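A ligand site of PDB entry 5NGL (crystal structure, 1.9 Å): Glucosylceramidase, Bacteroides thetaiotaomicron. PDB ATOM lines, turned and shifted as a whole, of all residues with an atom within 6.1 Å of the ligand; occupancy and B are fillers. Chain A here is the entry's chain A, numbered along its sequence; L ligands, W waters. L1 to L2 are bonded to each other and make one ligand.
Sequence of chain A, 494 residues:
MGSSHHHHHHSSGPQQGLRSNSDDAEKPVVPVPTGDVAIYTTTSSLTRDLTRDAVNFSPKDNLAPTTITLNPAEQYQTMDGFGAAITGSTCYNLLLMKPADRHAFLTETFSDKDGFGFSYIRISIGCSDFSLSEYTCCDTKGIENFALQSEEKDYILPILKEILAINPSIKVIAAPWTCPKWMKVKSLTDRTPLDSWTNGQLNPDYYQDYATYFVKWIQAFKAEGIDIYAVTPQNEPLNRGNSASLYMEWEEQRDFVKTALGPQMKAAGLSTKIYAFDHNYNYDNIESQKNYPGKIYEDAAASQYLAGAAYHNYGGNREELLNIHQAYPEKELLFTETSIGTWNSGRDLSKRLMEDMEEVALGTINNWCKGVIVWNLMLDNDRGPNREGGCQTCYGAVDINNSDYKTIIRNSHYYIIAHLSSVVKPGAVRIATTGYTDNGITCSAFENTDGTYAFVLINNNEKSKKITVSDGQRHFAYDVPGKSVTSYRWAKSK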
ATOM      1  N   ARG A 122      -6.999 -17.180  19.223  1.00  0.00           N
ATOM      2  CA  ARG A 122      -7.941 -16.427  18.402  1.00  0.00           C
ATOM      3  C   ARG A 122      -9.243 -16.210  19.174  1.00  0.00           C
ATOM      4  O   ARG A 122      -9.726 -17.126  19.849  1.00  0.00           O
ATOM      5  CB  ARG A 122      -8.181 -17.184  17.112  1.00  0.00           C
ATOM      6  CG  ARG A 122      -9.147 -16.554  16.125  1.00  0.00           C
ATOM      7  CD  ARG A 122      -8.820 -17.042  14.698  1.00  0.00           C
ATOM      8  NE  ARG A 122      -9.740 -16.541  13.653  1.00  0.00           N
ATOM      9  CZ  ARG A 122     -10.840 -17.165  13.209  1.00  0.00           C
ATOM     10  NH1 ARG A 122     -11.255 -18.335  13.702  1.00  0.00           N
ATOM     11  NH2 ARG A 122     -11.565 -16.589  12.241  1.00  0.00           N
ATOM     12  N   SER A 128     -19.384 -15.230  18.312  1.00  0.00           N
ATOM     13  CA  SER A 128     -19.212 -16.234  17.257  1.00  0.00           C
ATOM     14  C   SER A 128     -20.322 -17.236  17.455  1.00  0.00           C
ATOM     15  O   SER A 128     -21.231 -17.019  18.274  1.00  0.00           O
ATOM     16  CB  SER A 128     -17.856 -16.913  17.335  1.00  0.00           C
ATOM     17  OG  SER A 128     -17.824 -17.800  18.422  1.00  0.00           O
ATOM     18  N   ASP A 129     -20.259 -18.360  16.733  1.00  0.00           N
ATOM     19  CA  ASP A 129     -21.193 -19.480  16.992  1.00  0.00           C
ATOM     20  C   ASP A 129     -20.851 -20.275  18.269  1.00  0.00           C
ATOM     21  O   ASP A 129     -21.598 -21.170  18.625  1.00  0.00           O
ATOM     22  CB  ASP A 129     -21.380 -20.416  15.791  1.00  0.00           C
ATOM     23  CG  ASP A 129     -20.100 -21.074  15.313  1.00  0.00           C
ATOM     24  OD1 ASP A 129     -19.006 -20.513  15.487  1.00  0.00           O
ATOM     25  OD2 ASP A 129     -20.206 -22.159  14.691  1.00  0.00           O
ATOM     26  N   PHE A 130     -19.780 -19.911  18.981  1.00  0.00           N
ATOM     27  CA  PHE A 130     -19.533 -20.434  20.297  1.00  0.00           C
ATOM     28  C   PHE A 130     -19.487 -19.352  21.395  1.00  0.00           C
ATOM     29  O   PHE A 130     -18.656 -19.366  22.336  1.00  0.00           O
ATOM     30  CB  PHE A 130     -18.291 -21.315  20.243  1.00  0.00           C
ATOM     31  CG  PHE A 130     -18.540 -22.595  19.519  1.00  0.00           C
ATOM     32  CD1 PHE A 130     -19.033 -23.716  20.204  1.00  0.00           C
ATOM     33  CD2 PHE A 130     -18.335 -22.692  18.154  1.00  0.00           C
ATOM     34  CE1 PHE A 130     -19.271 -24.914  19.555  1.00  0.00           C
ATOM     35  CE2 PHE A 130     -18.582 -23.909  17.492  1.00  0.00           C
ATOM     36  CZ  PHE A 130     -19.034 -25.007  18.193  1.00  0.00           C
ATOM     37  N   TRP A 177     -17.629 -11.996  13.618  1.00  0.00           N
ATOM     38  CA  TRP A 177     -18.468 -12.917  12.836  1.00  0.00           C
ATOM     39  C   TRP A 177     -19.591 -12.123  12.142  1.00  0.00           C
ATOM     40  O   TRP A 177     -20.024 -12.498  11.049  1.00  0.00           O
ATOM     41  CB  TRP A 177     -19.030 -14.059  13.733  1.00  0.00           C
ATOM     42  CG  TRP A 177     -18.190 -15.329  13.720  1.00  0.00           C
ATOM     43  CD1 TRP A 177     -18.608 -16.577  13.326  1.00  0.00           C
ATOM     44  CD2 TRP A 177     -16.819 -15.493  14.139  1.00  0.00           C
ATOM     45  NE1 TRP A 177     -17.599 -17.501  13.469  1.00  0.00           N
ATOM     46  CE2 TRP A 177     -16.478 -16.857  13.954  1.00  0.00           C
ATOM     47  CE3 TRP A 177     -15.847 -14.618  14.642  1.00  0.00           C
ATOM     48  CZ2 TRP A 177     -15.202 -17.361  14.236  1.00  0.00           C
ATOM     49  CZ3 TRP A 177     -14.571 -15.125  14.957  1.00  0.00           C
ATOM     50  CH2 TRP A 177     -14.251 -16.478  14.719  1.00  0.00           C
ATOM     51  N   ASN A 235     -14.706 -12.832   9.821  1.00  0.00           N
ATOM     52  CA  ASN A 235     -14.584 -14.274   9.723  1.00  0.00           C
ATOM     53  C   ASN A 235     -15.295 -14.859   8.494  1.00  0.00           C
ATOM     54  O   ASN A 235     -16.505 -14.656   8.326  1.00  0.00           O
ATOM     55  CB  ASN A 235     -15.181 -14.943  10.931  1.00  0.00           C
ATOM     56  CG  ASN A 235     -15.075 -16.418  10.861  1.00  0.00           C
ATOM     57  OD1 ASN A 235     -13.971 -16.942  10.897  1.00  0.00           O
ATOM     58  ND2 ASN A 235     -16.238 -17.132  10.744  1.00  0.00           N
ATOM     59  N   GLU A 236     -14.565 -15.613   7.669  1.00  0.00           N
ATOM     60  CA  GLU A 236     -15.197 -16.394   6.585  1.00  0.00           C
ATOM     61  C   GLU A 236     -16.147 -15.520   5.763  1.00  0.00           C
ATOM     62  O   GLU A 236     -17.338 -15.782   5.689  1.00  0.00           O
ATOM     63  CB  GLU A 236     -15.937 -17.560   7.190  1.00  0.00           C
ATOM     64  CG  GLU A 236     -15.019 -18.537   7.931  1.00  0.00           C
ATOM     65  CD  GLU A 236     -15.464 -19.988   7.843  1.00  0.00           C
ATOM     66  OE1 GLU A 236     -16.673 -20.232   7.913  1.00  0.00           O
ATOM     67  OE2 GLU A 236     -14.590 -20.903   7.787  1.00  0.00           O
ATOM     68  N   ASN A 239     -19.029 -16.825   3.620  1.00  0.00           N
ATOM     69  CA  ASN A 239     -20.113 -17.600   4.204  1.00  0.00           C
ATOM     70  C   ASN A 239     -21.300 -16.689   4.574  1.00  0.00           C
ATOM     71  O   ASN A 239     -21.111 -15.694   5.271  1.00  0.00           O
ATOM     72  CB  ASN A 239     -19.605 -18.391   5.422  1.00  0.00           C
ATOM     73  CG  ASN A 239     -20.661 -19.272   6.026  1.00  0.00           C
ATOM     74  OD1 ASN A 239     -21.628 -19.656   5.359  1.00  0.00           O
ATOM     75  ND2 ASN A 239     -20.495 -19.610   7.284  1.00  0.00           N
ATOM     76  N   ASN A 242     -24.165 -19.966   9.073  1.00  0.00           N
ATOM     77  CA  ASN A 242     -23.713 -19.911  10.458  1.00  0.00           C
ATOM     78  C   ASN A 242     -24.822 -19.276  11.282  1.00  0.00           C
ATOM     79  O   ASN A 242     -25.938 -19.044  10.761  1.00  0.00           O
ATOM     80  CB  ASN A 242     -22.333 -19.168  10.567  1.00  0.00           C
ATOM     81  CG  ASN A 242     -21.444 -19.666  11.718  1.00  0.00           C
ATOM     82  OD1 ASN A 242     -21.935 -20.240  12.671  1.00  0.00           O
ATOM     83  ND2 ASN A 242     -20.140 -19.392  11.642  1.00  0.00           N
ATOM     84  N   HIS A 312      -8.465 -20.828   6.318  1.00  0.00           N
ATOM     85  CA  HIS A 312      -9.030 -22.009   6.901  1.00  0.00           C
ATOM     86  C   HIS A 312      -8.973 -23.163   5.862  1.00  0.00           C
ATOM     87  O   HIS A 312      -8.706 -22.949   4.666  1.00  0.00           O
ATOM     88  CB  HIS A 312     -10.503 -21.781   7.284  1.00  0.00           C
ATOM     89  CG  HIS A 312     -10.795 -20.571   8.131  1.00  0.00           C
ATOM     90  ND1 HIS A 312     -12.072 -20.209   8.468  1.00  0.00           N
ATOM     91  CD2 HIS A 312      -9.985 -19.634   8.682  1.00  0.00           C
ATOM     92  CE1 HIS A 312     -12.045 -19.115   9.220  1.00  0.00           C
ATOM     93  NE2 HIS A 312     -10.790 -18.750   9.357  1.00  0.00           N
ATOM     94  N   TYR A 314     -11.553 -25.609   5.385  1.00  0.00           N
ATOM     95  CA  TYR A 314     -12.842 -26.287   5.322  1.00  0.00           C
ATOM     96  C   TYR A 314     -13.252 -26.612   3.908  1.00  0.00           C
ATOM     97  O   TYR A 314     -14.201 -27.358   3.721  1.00  0.00           O
ATOM     98  CB  TYR A 314     -13.945 -25.490   6.018  1.00  0.00           C
ATOM     99  CG  TYR A 314     -13.730 -25.285   7.487  1.00  0.00           C
ATOM    100  CD1 TYR A 314     -14.013 -26.293   8.406  1.00  0.00           C
ATOM    101  CD2 TYR A 314     -13.246 -24.072   7.978  1.00  0.00           C
ATOM    102  CE1 TYR A 314     -13.829 -26.095   9.776  1.00  0.00           C
ATOM    103  CE2 TYR A 314     -13.049 -23.869   9.343  1.00  0.00           C
ATOM    104  CZ  TYR A 314     -13.333 -24.861  10.238  1.00  0.00           C
ATOM    105  OH  TYR A 314     -13.108 -24.615  11.590  1.00  0.00           O
ATOM    106  N   GLU A 337      -8.000 -21.134  11.281  1.00  0.00           N
ATOM    107  CA  GLU A 337      -9.091 -21.983  11.771  1.00  0.00           C
ATOM    108  C   GLU A 337      -9.254 -23.326  11.044  1.00  0.00           C
ATOM    109  O   GLU A 337      -9.247 -23.385   9.821  1.00  0.00           O
ATOM    110  CB  GLU A 337     -10.426 -21.260  11.731  1.00  0.00           C
ATOM    111  CG  GLU A 337     -11.429 -21.784  12.779  1.00  0.00           C
ATOM    112  CD  GLU A 337     -12.885 -21.389  12.526  1.00  0.00           C
ATOM    113  OE1 GLU A 337     -13.234 -20.174  12.632  1.00  0.00           O
ATOM    114  OE2 GLU A 337     -13.702 -22.318  12.234  1.00  0.00           O
ATOM    115  N   SER A 339     -11.517 -27.274  12.253  1.00  0.00           N
ATOM    116  CA  SER A 339     -12.339 -27.950  13.268  1.00  0.00           C
ATOM    117  C   SER A 339     -12.313 -29.476  13.103  1.00  0.00           C
ATOM    118  O   SER A 339     -12.041 -30.012  12.015  1.00  0.00           O
ATOM    119  CB  SER A 339     -13.807 -27.533  13.205  1.00  0.00           C
ATOM    120  OG  SER A 339     -14.041 -26.260  13.714  1.00  0.00           O
ATOM    121  N   TRP A 343     -18.520 -34.999  11.455  1.00  0.00           N
ATOM    122  CA  TRP A 343     -18.256 -35.200  10.024  1.00  0.00           C
ATOM    123  C   TRP A 343     -16.896 -35.824   9.664  1.00  0.00           C
ATOM    124  O   TRP A 343     -16.738 -36.254   8.531  1.00  0.00           O
ATOM    125  CB  TRP A 343     -18.417 -33.878   9.265  1.00  0.00           C
ATOM    126  CG  TRP A 343     -17.325 -32.887   9.572  1.00  0.00           C
ATOM    127  CD1 TRP A 343     -16.141 -32.740   8.921  1.00  0.00           C
ATOM    128  CD2 TRP A 343     -17.338 -31.902  10.619  1.00  0.00           C
ATOM    129  NE1 TRP A 343     -15.395 -31.764   9.518  1.00  0.00           N
ATOM    130  CE2 TRP A 343     -16.105 -31.228  10.551  1.00  0.00           C
ATOM    131  CE3 TRP A 343     -18.258 -31.560  11.631  1.00  0.00           C
ATOM    132  CZ2 TRP A 343     -15.765 -30.203  11.440  1.00  0.00           C
ATOM    133  CZ3 TRP A 343     -17.910 -30.530  12.523  1.00  0.00           C
ATOM    134  CH2 TRP A 343     -16.662 -29.889  12.431  1.00  0.00           C
ATOM    135  N   TRP A 375      -9.734 -24.247  16.183  1.00  0.00           N
ATOM    136  CA  TRP A 375     -10.912 -23.665  16.666  1.00  0.00           C
ATOM    137  C   TRP A 375     -11.079 -23.902  18.201  1.00  0.00           C
ATOM    138  O   TRP A 375     -10.087 -23.805  18.941  1.00  0.00           O
ATOM    139  CB  TRP A 375     -12.073 -24.153  15.773  1.00  0.00           C
ATOM    140  CG  TRP A 375     -13.405 -23.425  15.876  1.00  0.00           C
ATOM    141  CD1 TRP A 375     -14.646 -23.977  15.693  1.00  0.00           C
ATOM    142  CD2 TRP A 375     -13.634 -22.037  16.172  1.00  0.00           C
ATOM    143  NE1 TRP A 375     -15.612 -23.025  15.838  1.00  0.00           N
ATOM    144  CE2 TRP A 375     -15.029 -21.830  16.132  1.00  0.00           C
ATOM    145  CE3 TRP A 375     -12.800 -20.932  16.416  1.00  0.00           C
ATOM    146  CZ2 TRP A 375     -15.615 -20.550  16.383  1.00  0.00           C
ATOM    147  CZ3 TRP A 375     -13.390 -19.674  16.677  1.00  0.00           C
ATOM    148  CH2 TRP A 375     -14.773 -19.501  16.656  1.00  0.00           C
ATOM    149  N   ASN A 376     -12.271 -24.126  18.702  1.00  0.00           N
ATOM    150  CA  ASN A 376     -12.507 -24.152  20.170  1.00  0.00           C
ATOM    151  C   ASN A 376     -11.461 -24.983  20.900  1.00  0.00           C
ATOM    152  O   ASN A 376     -11.253 -26.177  20.560  1.00  0.00           O
ATOM    153  CB  ASN A 376     -13.823 -24.765  20.526  1.00  0.00           C
ATOM    154  CG  ASN A 376     -14.995 -23.948  20.049  1.00  0.00           C
ATOM    155  OD1 ASN A 376     -15.411 -23.030  20.734  1.00  0.00           O
ATOM    156  ND2 ASN A 376     -15.552 -24.323  18.870  1.00  0.00           N
ATOM    157  N   GLY A 389     -28.254 -22.955  14.600  1.00  0.00           N
ATOM    158  CA  GLY A 389     -27.762 -22.479  13.317  1.00  0.00           C
ATOM    159  C   GLY A 389     -26.236 -22.450  13.211  1.00  0.00           C
ATOM    160  O   GLY A 389     -25.718 -22.284  12.124  1.00  0.00           O
ATOM    161  N   GLY A 390     -25.541 -22.581  14.331  1.00  0.00           N
ATOM    162  CA  GLY A 390     -24.059 -22.605  14.318  1.00  0.00           C
ATOM    163  C   GLY A 390     -23.600 -24.038  14.308  1.00  0.00           C
ATOM    164  O   GLY A 390     -24.431 -24.963  14.139  1.00  0.00           O
ATOM    165  N   CYS A 391     -22.304 -24.275  14.493  1.00  0.00           N
ATOM    166  CA  CYS A 391     -21.857 -25.662  14.507  1.00  0.00           C
ATOM    167  C   CYS A 391     -22.388 -26.369  15.756  1.00  0.00           C
ATOM    168  O   CYS A 391     -22.085 -25.975  16.847  1.00  0.00           O
ATOM    169  CB  CYS A 391     -20.348 -25.779  14.436  1.00  0.00           C
ATOM    170  SG  CYS A 391     -19.828 -27.521  14.309  1.00  0.00           S
ATOM    171  N   GLN A 392     -23.191 -27.398  15.574  1.00  0.00           N
ATOM    172  CA  GLN A 392     -23.653 -28.250  16.667  1.00  0.00           C
ATOM    173  C   GLN A 392     -23.111 -29.679  16.529  1.00  0.00           C
ATOM    174  O   GLN A 392     -23.520 -30.577  17.267  1.00  0.00           O
ATOM    175  CB  GLN A 392     -25.175 -28.196  16.737  1.00  0.00           C
ATOM    176  CG  GLN A 392     -25.684 -26.781  17.065  1.00  0.00           C
ATOM    177  CD  GLN A 392     -27.152 -26.713  17.352  1.00  0.00           C
ATOM    178  OE1 GLN A 392     -27.968 -26.823  16.427  1.00  0.00           O
ATOM    179  NE2 GLN A 392     -27.513 -26.531  18.623  1.00  0.00           N
ATOM    180  N   THR A 393     -22.159 -29.867  15.617  1.00  0.00           N
ATOM    181  CA  THR A 393     -21.504 -31.132  15.385  1.00  0.00           C
ATOM    182  C   THR A 393     -20.007 -31.098  15.690  1.00  0.00           C
ATOM    183  O   THR A 393     -19.297 -32.056  15.372  1.00  0.00           O
ATOM    184  CB  THR A 393     -21.659 -31.554  13.890  1.00  0.00           C
ATOM    185  OG1 THR A 393     -21.309 -30.475  13.038  1.00  0.00           O
ATOM    186  CG2 THR A 393     -23.105 -32.007  13.624  1.00  0.00           C
ATOM    187  N   CYS A 394     -19.513 -30.015  16.314  1.00  0.00           N
ATOM    188  CA  CYS A 394     -18.082 -29.830  16.538  1.00  0.00           C
ATOM    189  C   CYS A 394     -17.586 -30.475  17.859  1.00  0.00           C
ATOM    190  O   CYS A 394     -18.322 -30.524  18.868  1.00  0.00           O
ATOM    191  CB  CYS A 394     -17.763 -28.314  16.578  1.00  0.00           C
ATOM    192  SG  CYS A 394     -17.818 -27.484  14.973  1.00  0.00           S
HETATM  193  C1  LIG L   1     -16.133 -22.154  10.322  1.00  0.00           C
HETATM  194  C2  LIG L   1     -16.691 -21.009  11.170  1.00  0.00           C
HETATM  195  O1  LIG L   1     -15.769 -19.889  11.102  1.00  0.00           O
HETATM  196  C3  LIG L   1     -16.951 -21.390  12.621  1.00  0.00           C
HETATM  197  O2  LIG L   1     -17.794 -20.403  13.153  1.00  0.00           O
HETATM  198  C4  LIG L   1     -17.621 -22.772  12.672  1.00  0.00           C
HETATM  199  O3  LIG L   1     -18.038 -23.125  13.989  1.00  0.00           O
HETATM  200  C5  LIG L   1     -16.668 -23.844  12.139  1.00  0.00           C
HETATM  201  N1  LIG L   1     -16.235 -23.502  10.797  1.00  0.00           N
HETATM  202  C6  LIG L   1     -17.308 -25.229  12.083  1.00  0.00           C
HETATM  203  O4  LIG L   1     -18.394 -25.260  11.114  1.00  0.00           O
HETATM  204  C1  LG2 L   2     -20.235 -26.290  10.297  1.00  0.00           C
HETATM  205  C2  LG2 L   2     -20.713 -27.620   9.740  1.00  0.00           C
HETATM  206  C3  LG2 L   2     -19.733 -28.198   8.759  1.00  0.00           C
HETATM  207  C4  LG2 L   2     -18.316 -28.247   9.363  1.00  0.00           C
HETATM  208  C5  LG2 L   2     -17.245 -28.727   8.381  1.00  0.00           C
HETATM  209  C6  LG2 L   2     -18.852 -26.483  10.885  1.00  0.00           C
HETATM  210  O1  LG2 L   2     -21.162 -25.827  11.308  1.00  0.00           O
HETATM  211  O2  LG2 L   2     -21.974 -27.454   9.096  1.00  0.00           O
HETATM  212  O3  LG2 L   2     -20.161 -29.537   8.464  1.00  0.00           O
HETATM  213  O4  LG2 L   2     -17.937 -26.950   9.880  1.00  0.00           O
HETATM  214  O5  LG2 L   2     -17.233 -27.844   7.247  1.00  0.00           O
HETATM  215  O   HOH W   1     -23.662 -23.734  10.941  1.00  0.00           O
HETATM  216  O   HOH W   2     -21.162 -22.920  11.683  1.00  0.00           O
HETATM  217  O   HOH W   3     -16.635 -24.659   8.400  1.00  0.00           O
HETATM  218  O   HOH W   4     -21.392 -31.197  10.409  1.00  0.00           O
HETATM  219  O   HOH W   5     -23.895 -26.523  10.905  1.00  0.00           O
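Merely in contact with the ligand: Phe 130 (3.6 Å), Ser 339 (3.8 Å), Trp 343 (3.5 Å) and Cys 394 (3.7 Å).
Hydrophobic or aromatic side chains that line the ligand: Phe 130, Trp 177, Tyr 314, Trp 343 and Trp 375.
Within 4 Å of the ligand: Asp 129, Phe 130, Trp 177, Asn 235, Glu 236, Asn 242, Tyr 314, Glu 337, Ser 339, Trp 343, Trp 375, Cys 391 and Cys 394.
The nearest printed residue that does not touch the ligand is His 312 (4.2 Å).
Water W4 bridges the side-chain hydroxyl (OG1) of Thr 393 (2.7 Å) and an oxygen (O3) of LG2 L2 (2.8 Å).
Water W2 lies within hydrogen-bond range of O1 of LG2 L2 (2.9 Å), OD1 of Asn 242 (3.0 Å), OD2 of Asp 129 (3.2 Å) and N of Cys 391 (3.3 Å).
Water W1 lies within hydrogen-bond range of O of Gly 389 (2.8 Å) and O1 of LG2 L2 (3.3 Å).
OD2 of Asp 129 sits close to OD1 of Asn 242, 3.3 Å away.
OD2 of Asp 129 sits at hydrogen-bond distance from N of Cys 391, at 3.0 Å.
OD1 of Asn 235 lies within hydrogen-bond range of NH2 of Arg 122, at 2.8 Å.
The side-chain hydroxyl (OH) of Tyr 314 is in hydrogen-bond range of the side-chain carboxylate (OE2) of Glu 337 (2.5 Å).
The indole nitrogen (NE1) of Trp 375 sits close to the side-chain amide nitrogen (ND2) of Asn 376.
The side-chain sulfur of Cys 391 sits at hydrogen-bond distance from the side-chain hydroxyl of Thr 393 (3.5 Å).
The side-chain hydroxyl (OG) of Ser 339 lies within hydrogen-bond range of the side-chain hydroxyl (OH) of Tyr 314 (2.8 Å).
The backbone NH (N) of Phe 130 is in hydrogen-bond range of the side-chain hydroxyl (OG) of Ser 128 (2.9 Å).
O3 of LIG L1 is in hydrogen-bond range of OD2 of Asp 129 (2.5 Å).
O1 of LIG L1 is in hydrogen-bond range of ND2 of Asn 235 (2.8 Å).
O2 of LIG L1 lies within hydrogen-bond range of NE1 of Trp 177 (2.9 Å).
ND2 of Asn 242 is in hydrogen-bond range of O2 of LIG L1 (3.0 Å).
OE2 of Glu 337 lies within salt-bridge range of N1 of LIG L1 (3.1 Å).
The indole nitrogen of Trp 375 lies within hydrogen-bond range of an oxygen (O3) of LIG L1, at 3.1 Å.
An oxygen (O1) of LIG L1 sits close to the side-chain carboxylate (OE1) of Glu 236.
The side-chain sulfur (SG) of Cys 391 sits close to an oxygen (O1) of LG2 L2 (3.7 Å).
OH of Tyr 314 lies close to N1 of LIG L1 (3.4 Å).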
